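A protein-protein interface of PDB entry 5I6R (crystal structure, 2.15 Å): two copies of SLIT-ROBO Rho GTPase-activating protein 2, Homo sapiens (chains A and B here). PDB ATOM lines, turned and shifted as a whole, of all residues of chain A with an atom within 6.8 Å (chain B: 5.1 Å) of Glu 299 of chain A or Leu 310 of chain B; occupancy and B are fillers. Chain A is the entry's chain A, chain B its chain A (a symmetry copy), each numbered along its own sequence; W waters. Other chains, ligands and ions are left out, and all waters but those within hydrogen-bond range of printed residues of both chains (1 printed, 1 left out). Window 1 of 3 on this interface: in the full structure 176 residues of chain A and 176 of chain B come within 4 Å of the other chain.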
ATOM      1  N   PHE A  53     -19.122   4.368  27.660  1.00  0.00           N
ATOM      2  CA  PHE A  53     -19.307   5.624  26.929  1.00  0.00           C
ATOM      3  C   PHE A  53     -19.008   6.885  27.742  1.00  0.00           C
ATOM      4  O   PHE A  53     -18.469   7.845  27.180  1.00  0.00           O
ATOM      5  CB  PHE A  53     -20.647   5.672  26.203  1.00  0.00           C
ATOM      6  CG  PHE A  53     -20.656   4.879  24.949  1.00  0.00           C
ATOM      7  CD1 PHE A  53     -20.034   5.383  23.772  1.00  0.00           C
ATOM      8  CD2 PHE A  53     -21.220   3.607  24.917  1.00  0.00           C
ATOM      9  CE1 PHE A  53     -20.013   4.624  22.597  1.00  0.00           C
ATOM     10  CE2 PHE A  53     -21.209   2.851  23.739  1.00  0.00           C
ATOM     11  CZ  PHE A  53     -20.607   3.352  22.586  1.00  0.00           C
ATOM     12  N   LYS A  56     -15.244   7.053  27.622  1.00  0.00           N
ATOM     13  CA  LYS A  56     -14.793   7.359  26.292  1.00  0.00           C
ATOM     14  C   LYS A  56     -15.068   8.838  25.983  1.00  0.00           C
ATOM     15  O   LYS A  56     -14.213   9.500  25.380  1.00  0.00           O
ATOM     16  CB  LYS A  56     -15.432   6.424  25.254  1.00  0.00           C
ATOM     17  CG  LYS A  56     -14.616   6.347  23.958  1.00  0.00           C
ATOM     18  CD  LYS A  56     -15.169   5.370  22.914  1.00  0.00           C
ATOM     19  CE  LYS A  56     -14.203   5.231  21.719  1.00  0.00           C
ATOM     20  NZ  LYS A  56     -14.038   6.502  20.924  1.00  0.00           N
ATOM     21  N   GLU A  60     -12.269  11.372  24.880  1.00  0.00           N
ATOM     22  CA  GLU A  60     -12.426  12.141  23.645  1.00  0.00           C
ATOM     23  C   GLU A  60     -12.281  13.667  23.839  1.00  0.00           C
ATOM     24  O   GLU A  60     -11.669  14.345  22.998  1.00  0.00           O
ATOM     25  CB  GLU A  60     -13.750  11.790  22.929  1.00  0.00           C
ATOM     26  CG  GLU A  60     -13.838  10.375  22.355  1.00  0.00           C
ATOM     27  CD  GLU A  60     -12.798  10.089  21.282  1.00  0.00           C
ATOM     28  OE1 GLU A  60     -12.362   8.924  21.147  1.00  0.00           O
ATOM     29  OE2 GLU A  60     -12.403  11.026  20.583  1.00  0.00           O
ATOM     30  N   HIS A 113     -13.955  15.682  17.637  1.00  0.00           N
ATOM     31  CA  HIS A 113     -13.897  14.886  18.855  1.00  0.00           C
ATOM     32  C   HIS A 113     -14.693  15.468  20.043  1.00  0.00           C
ATOM     33  O   HIS A 113     -15.141  14.704  20.891  1.00  0.00           O
ATOM     34  CB  HIS A 113     -12.455  14.567  19.213  1.00  0.00           C
ATOM     35  CG  HIS A 113     -11.811  13.620  18.255  1.00  0.00           C
ATOM     36  ND1 HIS A 113     -11.841  12.254  18.427  1.00  0.00           N
ATOM     37  CD2 HIS A 113     -11.114  13.839  17.117  1.00  0.00           C
ATOM     38  CE1 HIS A 113     -11.184  11.671  17.447  1.00  0.00           C
ATOM     39  NE2 HIS A 113     -10.741  12.609  16.631  1.00  0.00           N
ATOM     40  N   LEU A 116     -18.089  14.364  19.119  1.00  0.00           N
ATOM     41  CA  LEU A 116     -18.178  12.963  19.496  1.00  0.00           C
ATOM     42  C   LEU A 116     -18.497  12.794  20.976  1.00  0.00           C
ATOM     43  O   LEU A 116     -19.388  12.026  21.349  1.00  0.00           O
ATOM     44  CB  LEU A 116     -16.884  12.273  19.140  1.00  0.00           C
ATOM     45  CG  LEU A 116     -16.900  10.762  19.006  1.00  0.00           C
ATOM     46  CD1 LEU A 116     -17.701  10.356  17.781  1.00  0.00           C
ATOM     47  CD2 LEU A 116     -15.469  10.265  18.894  1.00  0.00           C
ATOM     48  N   TYR A 120     -21.853  11.191  22.681  1.00  0.00           N
ATOM     49  CA  TYR A 120     -21.799  10.192  23.734  1.00  0.00           C
ATOM     50  C   TYR A 120     -22.611  10.650  24.943  1.00  0.00           C
ATOM     51  O   TYR A 120     -23.484   9.908  25.398  1.00  0.00           O
ATOM     52  CB  TYR A 120     -20.368   9.847  24.159  1.00  0.00           C
ATOM     53  CG  TYR A 120     -19.495   9.175  23.112  1.00  0.00           C
ATOM     54  CD1 TYR A 120     -20.033   8.665  21.921  1.00  0.00           C
ATOM     55  CD2 TYR A 120     -18.117   9.034  23.331  1.00  0.00           C
ATOM     56  CE1 TYR A 120     -19.224   8.054  20.977  1.00  0.00           C
ATOM     57  CE2 TYR A 120     -17.301   8.415  22.389  1.00  0.00           C
ATOM     58  CZ  TYR A 120     -17.868   7.927  21.221  1.00  0.00           C
ATOM     59  OH  TYR A 120     -17.072   7.331  20.290  1.00  0.00           O
ATOM     60  N   THR A 294     -26.090   4.669  16.469  1.00  0.00           N
ATOM     61  CA  THR A 294     -25.779   6.071  16.747  1.00  0.00           C
ATOM     62  C   THR A 294     -24.271   6.203  16.910  1.00  0.00           C
ATOM     63  O   THR A 294     -23.666   7.115  16.354  1.00  0.00           O
ATOM     64  CB  THR A 294     -26.522   6.583  17.991  1.00  0.00           C
ATOM     65  OG1 THR A 294     -27.910   6.290  17.838  1.00  0.00           O
ATOM     66  CG2 THR A 294     -26.336   8.091  18.168  1.00  0.00           C
ATOM     67  N   PHE A 295     -23.677   5.264  17.640  1.00  0.00           N
ATOM     68  CA  PHE A 295     -22.233   5.157  17.740  1.00  0.00           C
ATOM     69  C   PHE A 295     -21.597   5.059  16.343  1.00  0.00           C
ATOM     70  O   PHE A 295     -20.694   5.847  16.016  1.00  0.00           O
ATOM     71  CB  PHE A 295     -21.830   3.977  18.648  1.00  0.00           C
ATOM     72  CG  PHE A 295     -20.398   3.570  18.506  1.00  0.00           C
ATOM     73  CD1 PHE A 295     -19.376   4.367  19.007  1.00  0.00           C
ATOM     74  CD2 PHE A 295     -20.058   2.378  17.847  1.00  0.00           C
ATOM     75  CE1 PHE A 295     -18.040   3.986  18.846  1.00  0.00           C
ATOM     76  CE2 PHE A 295     -18.722   2.009  17.666  1.00  0.00           C
ATOM     77  CZ  PHE A 295     -17.719   2.798  18.190  1.00  0.00           C
ATOM     78  N   LEU A 296     -22.094   4.134  15.520  1.00  0.00           N
ATOM     79  CA  LEU A 296     -21.524   3.949  14.174  1.00  0.00           C
ATOM     80  C   LEU A 296     -21.644   5.179  13.261  1.00  0.00           C
ATOM     81  O   LEU A 296     -20.703   5.495  12.516  1.00  0.00           O
ATOM     82  CB  LEU A 296     -22.078   2.687  13.501  1.00  0.00           C
ATOM     83  CG  LEU A 296     -21.667   1.371  14.167  1.00  0.00           C
ATOM     84  CD1 LEU A 296     -22.640   0.279  13.729  1.00  0.00           C
ATOM     85  CD2 LEU A 296     -20.210   0.991  13.894  1.00  0.00           C
ATOM     86  N   SER A 297     -22.794   5.852  13.328  1.00  0.00           N
ATOM     87  CA  SER A 297     -23.041   7.087  12.592  1.00  0.00           C
ATOM     88  C   SER A 297     -22.059   8.190  12.989  1.00  0.00           C
ATOM     89  O   SER A 297     -21.468   8.811  12.117  1.00  0.00           O
ATOM     90  CB  SER A 297     -24.478   7.555  12.800  1.00  0.00           C
ATOM     91  OG  SER A 297     -24.674   8.858  12.231  1.00  0.00           O
ATOM     92  N   ALA A 298     -21.909   8.428  14.298  1.00  0.00           N
ATOM     93  CA  ALA A 298     -20.924   9.358  14.852  1.00  0.00           C
ATOM     94  C   ALA A 298     -19.508   9.100  14.313  1.00  0.00           C
ATOM     95  O   ALA A 298     -18.860  10.040  13.833  1.00  0.00           O
ATOM     96  CB  ALA A 298     -20.949   9.318  16.370  1.00  0.00           C
ATOM     97  N   GLU A 299     -19.065   7.829  14.344  1.00  0.00           N
ATOM     98  CA  GLU A 299     -17.751   7.432  13.835  1.00  0.00           C
ATOM     99  C   GLU A 299     -17.597   7.640  12.326  1.00  0.00           C
ATOM    100  O   GLU A 299     -16.596   8.227  11.886  1.00  0.00           O
ATOM    101  CB  GLU A 299     -17.412   5.974  14.185  1.00  0.00           C
ATOM    102  CG  GLU A 299     -17.240   5.660  15.672  1.00  0.00           C
ATOM    103  CD  GLU A 299     -16.163   6.467  16.387  1.00  0.00           C
ATOM    104  OE1 GLU A 299     -16.180   6.452  17.627  1.00  0.00           O
ATOM    105  OE2 GLU A 299     -15.308   7.127  15.756  1.00  0.00           O
ATOM    106  N   LEU A 300     -18.569   7.146  11.551  1.00  0.00           N
ATOM    107  CA  LEU A 300     -18.597   7.340  10.109  1.00  0.00           C
ATOM    108  C   LEU A 300     -18.448   8.839   9.758  1.00  0.00           C
ATOM    109  O   LEU A 300     -17.655   9.194   8.880  1.00  0.00           O
ATOM    110  CB  LEU A 300     -19.884   6.737   9.508  1.00  0.00           C
ATOM    111  CG  LEU A 300     -20.196   6.953   8.018  1.00  0.00           C
ATOM    112  CD1 LEU A 300     -19.601   5.850   7.148  1.00  0.00           C
ATOM    113  CD2 LEU A 300     -21.694   7.107   7.759  1.00  0.00           C
ATOM    114  N   ASN A 301     -19.181   9.701  10.460  1.00  0.00           N
ATOM    115  CA  ASN A 301     -19.140  11.138  10.187  1.00  0.00           C
ATOM    116  C   ASN A 301     -17.799  11.786  10.529  1.00  0.00           C
ATOM    117  O   ASN A 301     -17.307  12.631   9.786  1.00  0.00           O
ATOM    118  CB  ASN A 301     -20.271  11.869  10.880  1.00  0.00           C
ATOM    119  CG  ASN A 301     -21.531  11.894  10.050  1.00  0.00           C
ATOM    120  OD1 ASN A 301     -21.639  12.671   9.105  1.00  0.00           O
ATOM    121  ND2 ASN A 301     -22.511  11.059  10.411  1.00  0.00           N
ATOM    122  N   LEU A 302     -17.214  11.376  11.648  1.00  0.00           N
ATOM    123  CA  LEU A 302     -15.892  11.867  12.038  1.00  0.00           C
ATOM    124  C   LEU A 302     -14.836  11.436  10.994  1.00  0.00           C
ATOM    125  O   LEU A 302     -14.006  12.235  10.579  1.00  0.00           O
ATOM    126  CB  LEU A 302     -15.570  11.439  13.476  1.00  0.00           C
ATOM    127  CG  LEU A 302     -14.263  11.890  14.121  1.00  0.00           C
ATOM    128  CD1 LEU A 302     -14.477  12.437  15.524  1.00  0.00           C
ATOM    129  CD2 LEU A 302     -13.394  10.661  14.189  1.00  0.00           C
ATOM    130  N   GLU A 303     -14.944  10.197  10.534  1.00  0.00           N
ATOM    131  CA  GLU A 303     -14.066   9.713   9.481  1.00  0.00           C
ATOM    132  C   GLU A 303     -14.256  10.463   8.158  1.00  0.00           C
ATOM    133  O   GLU A 303     -13.277  10.757   7.505  1.00  0.00           O
ATOM    134  CB  GLU A 303     -14.170   8.191   9.321  1.00  0.00           C
ATOM    135  CG  GLU A 303     -13.581   7.449  10.520  1.00  0.00           C
ATOM    136  CD  GLU A 303     -12.206   7.979  10.897  1.00  0.00           C
ATOM    137  OE1 GLU A 303     -12.048   8.464  12.037  1.00  0.00           O
ATOM    138  OE2 GLU A 303     -11.285   7.927  10.046  1.00  0.00           O
ATOM    139  N   GLN A 304     -15.490  10.813   7.792  1.00  0.00           N
ATOM    140  CA  GLN A 304     -15.722  11.582   6.575  1.00  0.00           C
ATOM    141  C   GLN A 304     -15.130  12.992   6.679  1.00  0.00           C
ATOM    142  O   GLN A 304     -14.487  13.481   5.741  1.00  0.00           O
ATOM    143  CB  GLN A 304     -17.204  11.653   6.238  1.00  0.00           C
ATOM    144  CG  GLN A 304     -17.716  10.482   5.405  1.00  0.00           C
ATOM    145  CD  GLN A 304     -19.240  10.414   5.352  1.00  0.00           C
ATOM    146  OE1 GLN A 304     -19.933  11.429   5.523  1.00  0.00           O
ATOM    147  NE2 GLN A 304     -19.769   9.212   5.119  1.00  0.00           N
ATOM    148  N   GLN B 105     -12.363  -3.034  19.139  1.00  0.00           N
ATOM    149  CA  GLN B 105     -12.140  -1.807  18.392  1.00  0.00           C
ATOM    150  C   GLN B 105     -11.314  -0.775  19.159  1.00  0.00           C
ATOM    151  O   GLN B 105     -10.461  -0.102  18.578  1.00  0.00           O
ATOM    152  CB  GLN B 105     -13.462  -1.203  17.971  1.00  0.00           C
ATOM    153  CG  GLN B 105     -13.413  -0.693  16.539  1.00  0.00           C
ATOM    154  CD  GLN B 105     -12.922   0.737  16.429  1.00  0.00           C
ATOM    155  OE1 GLN B 105     -12.374   1.132  15.387  1.00  0.00           O
ATOM    156  NE2 GLN B 105     -13.142   1.542  17.492  1.00  0.00           N
ATOM    157  N   LYS B 306      -9.259   1.528  11.267  1.00  0.00           N
ATOM    158  CA  LYS B 306     -10.448   1.903  12.025  1.00  0.00           C
ATOM    159  C   LYS B 306     -11.711   1.443  11.293  1.00  0.00           C
ATOM    160  O   LYS B 306     -12.610   0.837  11.908  1.00  0.00           O
ATOM    161  CB  LYS B 306     -10.482   3.407  12.301  1.00  0.00           C
ATOM    162  CG  LYS B 306     -11.493   3.836  13.349  1.00  0.00           C
ATOM    163  CD  LYS B 306     -11.588   5.353  13.406  1.00  0.00           C
ATOM    164  CE  LYS B 306     -12.662   5.809  14.390  1.00  0.00           C
ATOM    165  NZ  LYS B 306     -12.554   7.257  14.733  1.00  0.00           N
ATOM    166  N   HIS B 307     -11.763   1.712   9.985  1.00  0.00           N
ATOM    167  CA  HIS B 307     -12.903   1.333   9.140  1.00  0.00           C
ATOM    168  C   HIS B 307     -13.210  -0.160   9.247  1.00  0.00           C
ATOM    169  O   HIS B 307     -14.385  -0.539   9.394  1.00  0.00           O
ATOM    170  CB  HIS B 307     -12.650   1.725   7.691  1.00  0.00           C
ATOM    171  CG  HIS B 307     -13.853   1.604   6.818  1.00  0.00           C
ATOM    172  ND1 HIS B 307     -14.890   2.514   6.852  1.00  0.00           N
ATOM    173  CD2 HIS B 307     -14.190   0.682   5.887  1.00  0.00           C
ATOM    174  CE1 HIS B 307     -15.808   2.163   5.967  1.00  0.00           C
ATOM    175  NE2 HIS B 307     -15.410   1.052   5.372  1.00  0.00           N
ATOM    176  N   GLU B 308     -12.152  -0.973   9.178  1.00  0.00           N
ATOM    177  CA  GLU B 308     -12.243  -2.418   9.375  1.00  0.00           C
ATOM    178  C   GLU B 308     -12.883  -2.769  10.718  1.00  0.00           C
ATOM    179  O   GLU B 308     -13.794  -3.604  10.778  1.00  0.00           O
ATOM    180  CB  GLU B 308     -10.860  -3.082   9.267  1.00  0.00           C
ATOM    181  CG  GLU B 308     -10.858  -4.550   9.675  1.00  0.00           C
ATOM    182  CD  GLU B 308      -9.656  -5.299   9.162  1.00  0.00           C
ATOM    183  OE1 GLU B 308      -9.822  -6.468   8.748  1.00  0.00           O
ATOM    184  OE2 GLU B 308      -8.546  -4.720   9.165  1.00  0.00           O
ATOM    185  N   GLY B 309     -12.403  -2.126  11.793  1.00  0.00           N
ATOM    186  CA  GLY B 309     -12.925  -2.322  13.132  1.00  0.00           C
ATOM    187  C   GLY B 309     -14.396  -2.008  13.207  1.00  0.00           C
ATOM    188  O   GLY B 309     -15.155  -2.835  13.669  1.00  0.00           O
ATOM    189  N   LEU B 310     -14.792  -0.828  12.733  1.00  0.00           N
ATOM    190  CA  LEU B 310     -16.188  -0.391  12.731  1.00  0.00           C
ATOM    191  C   LEU B 310     -17.113  -1.279  11.879  1.00  0.00           C
ATOM    192  O   LEU B 310     -18.290  -1.426  12.217  1.00  0.00           O
ATOM    193  CB  LEU B 310     -16.307   1.067  12.248  1.00  0.00           C
ATOM    194  CG  LEU B 310     -15.582   2.137  13.056  1.00  0.00           C
ATOM    195  CD1 LEU B 310     -15.591   3.438  12.285  1.00  0.00           C
ATOM    196  CD2 LEU B 310     -16.201   2.316  14.446  1.00  0.00           C
ATOM    197  N   ASP B 311     -16.588  -1.842  10.785  1.00  0.00           N
ATOM    198  CA  ASP B 311     -17.337  -2.791   9.961  1.00  0.00           C
ATOM    199  C   ASP B 311     -17.655  -4.091  10.736  1.00  0.00           C
ATOM    200  O   ASP B 311     -18.745  -4.664  10.603  1.00  0.00           O
ATOM    201  CB  ASP B 311     -16.560  -3.108   8.677  1.00  0.00           C
ATOM    202  CG  ASP B 311     -17.301  -4.070   7.769  1.00  0.00           C
ATOM    203  OD1 ASP B 311     -18.257  -3.619   7.112  1.00  0.00           O
ATOM    204  OD2 ASP B 311     -16.941  -5.275   7.739  1.00  0.00           O
ATOM    205  N   ALA B 312     -16.702  -4.557  11.540  1.00  0.00           N
ATOM    206  CA  ALA B 312     -16.910  -5.738  12.367  1.00  0.00           C
ATOM    207  C   ALA B 312     -18.022  -5.510  13.433  1.00  0.00           C
ATOM    208  O   ALA B 312     -18.813  -6.407  13.721  1.00  0.00           O
ATOM    209  CB  ALA B 312     -15.598  -6.153  13.016  1.00  0.00           C
ATOM    210  N   ILE B 313     -18.092  -4.296  13.973  1.00  0.00           N
ATOM    211  CA  ILE B 313     -19.149  -3.907  14.902  1.00  0.00           C
ATOM    212  C   ILE B 313     -20.484  -3.812  14.174  1.00  0.00           C
ATOM    213  O   ILE B 313     -21.502  -4.253  14.697  1.00  0.00           O
ATOM    214  CB  ILE B 313     -18.836  -2.576  15.624  1.00  0.00           C
ATOM    215  CG1 ILE B 313     -17.532  -2.707  16.412  1.00  0.00           C
ATOM    216  CG2 ILE B 313     -19.966  -2.178  16.581  1.00  0.00           C
ATOM    217  CD1 ILE B 313     -16.959  -1.385  16.859  1.00  0.00           C
ATOM    218  N   GLU B 314     -20.482  -3.233  12.980  1.00  0.00           N
ATOM    219  CA  GLU B 314     -21.696  -3.162  12.177  1.00  0.00           C
ATOM    220  C   GLU B 314     -22.263  -4.535  11.827  1.00  0.00           C
ATOM    221  O   GLU B 314     -23.468  -4.736  11.921  1.00  0.00           O
ATOM    222  CB  GLU B 314     -21.519  -2.312  10.934  1.00  0.00           C
ATOM    223  CG  GLU B 314     -22.840  -1.696  10.494  1.00  0.00           C
ATOM    224  CD  GLU B 314     -22.837  -1.131   9.085  1.00  0.00           C
ATOM    225  OE1 GLU B 314     -23.850  -0.492   8.731  1.00  0.00           O
ATOM    226  OE2 GLU B 314     -21.855  -1.336   8.326  1.00  0.00           O
HETATM  227  O   HOH W   1     -12.720   8.853  17.726  1.00  0.00           O
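The side-chain amino group (NZ) of Lys 306 of chain B is in salt-bridge range of the side-chain carboxylate (OE1) of Glu 303 of chain A (3.0 Å).
The side-chain amino group of Lys 306 of chain B lies within salt-bridge range of the side-chain carboxylate of Glu 299 of chain A (2.9 Å).
The side-chain amino group (NZ) of Lys 56 of chain A lies within salt-bridge range of the side-chain carboxylate (OE1) of Glu 299 of chain A (3.9 Å).
The side-chain hydroxyl of Tyr 120 of chain A lies within hydrogen-bond range of the side-chain carboxylate of Glu 299 of chain A (2.9 Å).
The side-chain amide oxygen of Gln 105 of chain B lies close to the backbone carbonyl oxygen of Lys 306 of chain B, at 3.5 Å.
CE2 of Phe 295 of chain A touches CD1 of Ile 313 of chain B, at 3.9 Å.
Leu 310 of chain B touches Leu 296 of chain A.
Glu 314 of chain B touches Leu 296 of chain A (CG to CD1, 3.8 Å).
CB of Glu 299 of chain A touches CD1 of Leu 310 of chain B (3.7 Å).
Lys 306 of chain B touches Leu 302 of chain A (NZ to CD2, 3.5 Å).
Of chain B, only Lys 306 (2.9 Å) and Leu 310 (3.7 Å) come within 4 Å of Glu 299 of chain A.
Printed residues of chain A within 4 Å of Leu 310 of chain B: Leu 296 and Glu 299.
Of the printed residues of chain B, Phe 295 of chain A touches Ile 313 (3.9 Å).
Printed residues of chain A within 4 Å of Ile 313 of chain B: Phe 295.
Of the printed residues of chain B, Leu 296 of chain A touches Leu 310 and Glu 314.
Leu 300 of chain A touches none of the printed residues of chain B.
Printed residues of chain A that touch a printed residue of chain B: Phe 295, Leu 296, Glu 299, Leu 302 and Glu 303.
Among the printed residues, 7 pairs touch across the chains.
Among the printed residues, Asp or Glu carboxylates within 4 Å of a Lys or Arg side-chain nitrogen of the other chain: Glu 299 of chain A with Lys 306 of chain B (2.9 Å) and Glu 303 of chain A with Lys 306 of chain B (3.0 Å).
No position is printed for both chains.
Water W1 lies within hydrogen-bond range of the side-chain amino group of Lys 306 of chain B (3.4 Å) and the side-chain carboxylate of Glu 60 of chain A (3.4 Å).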
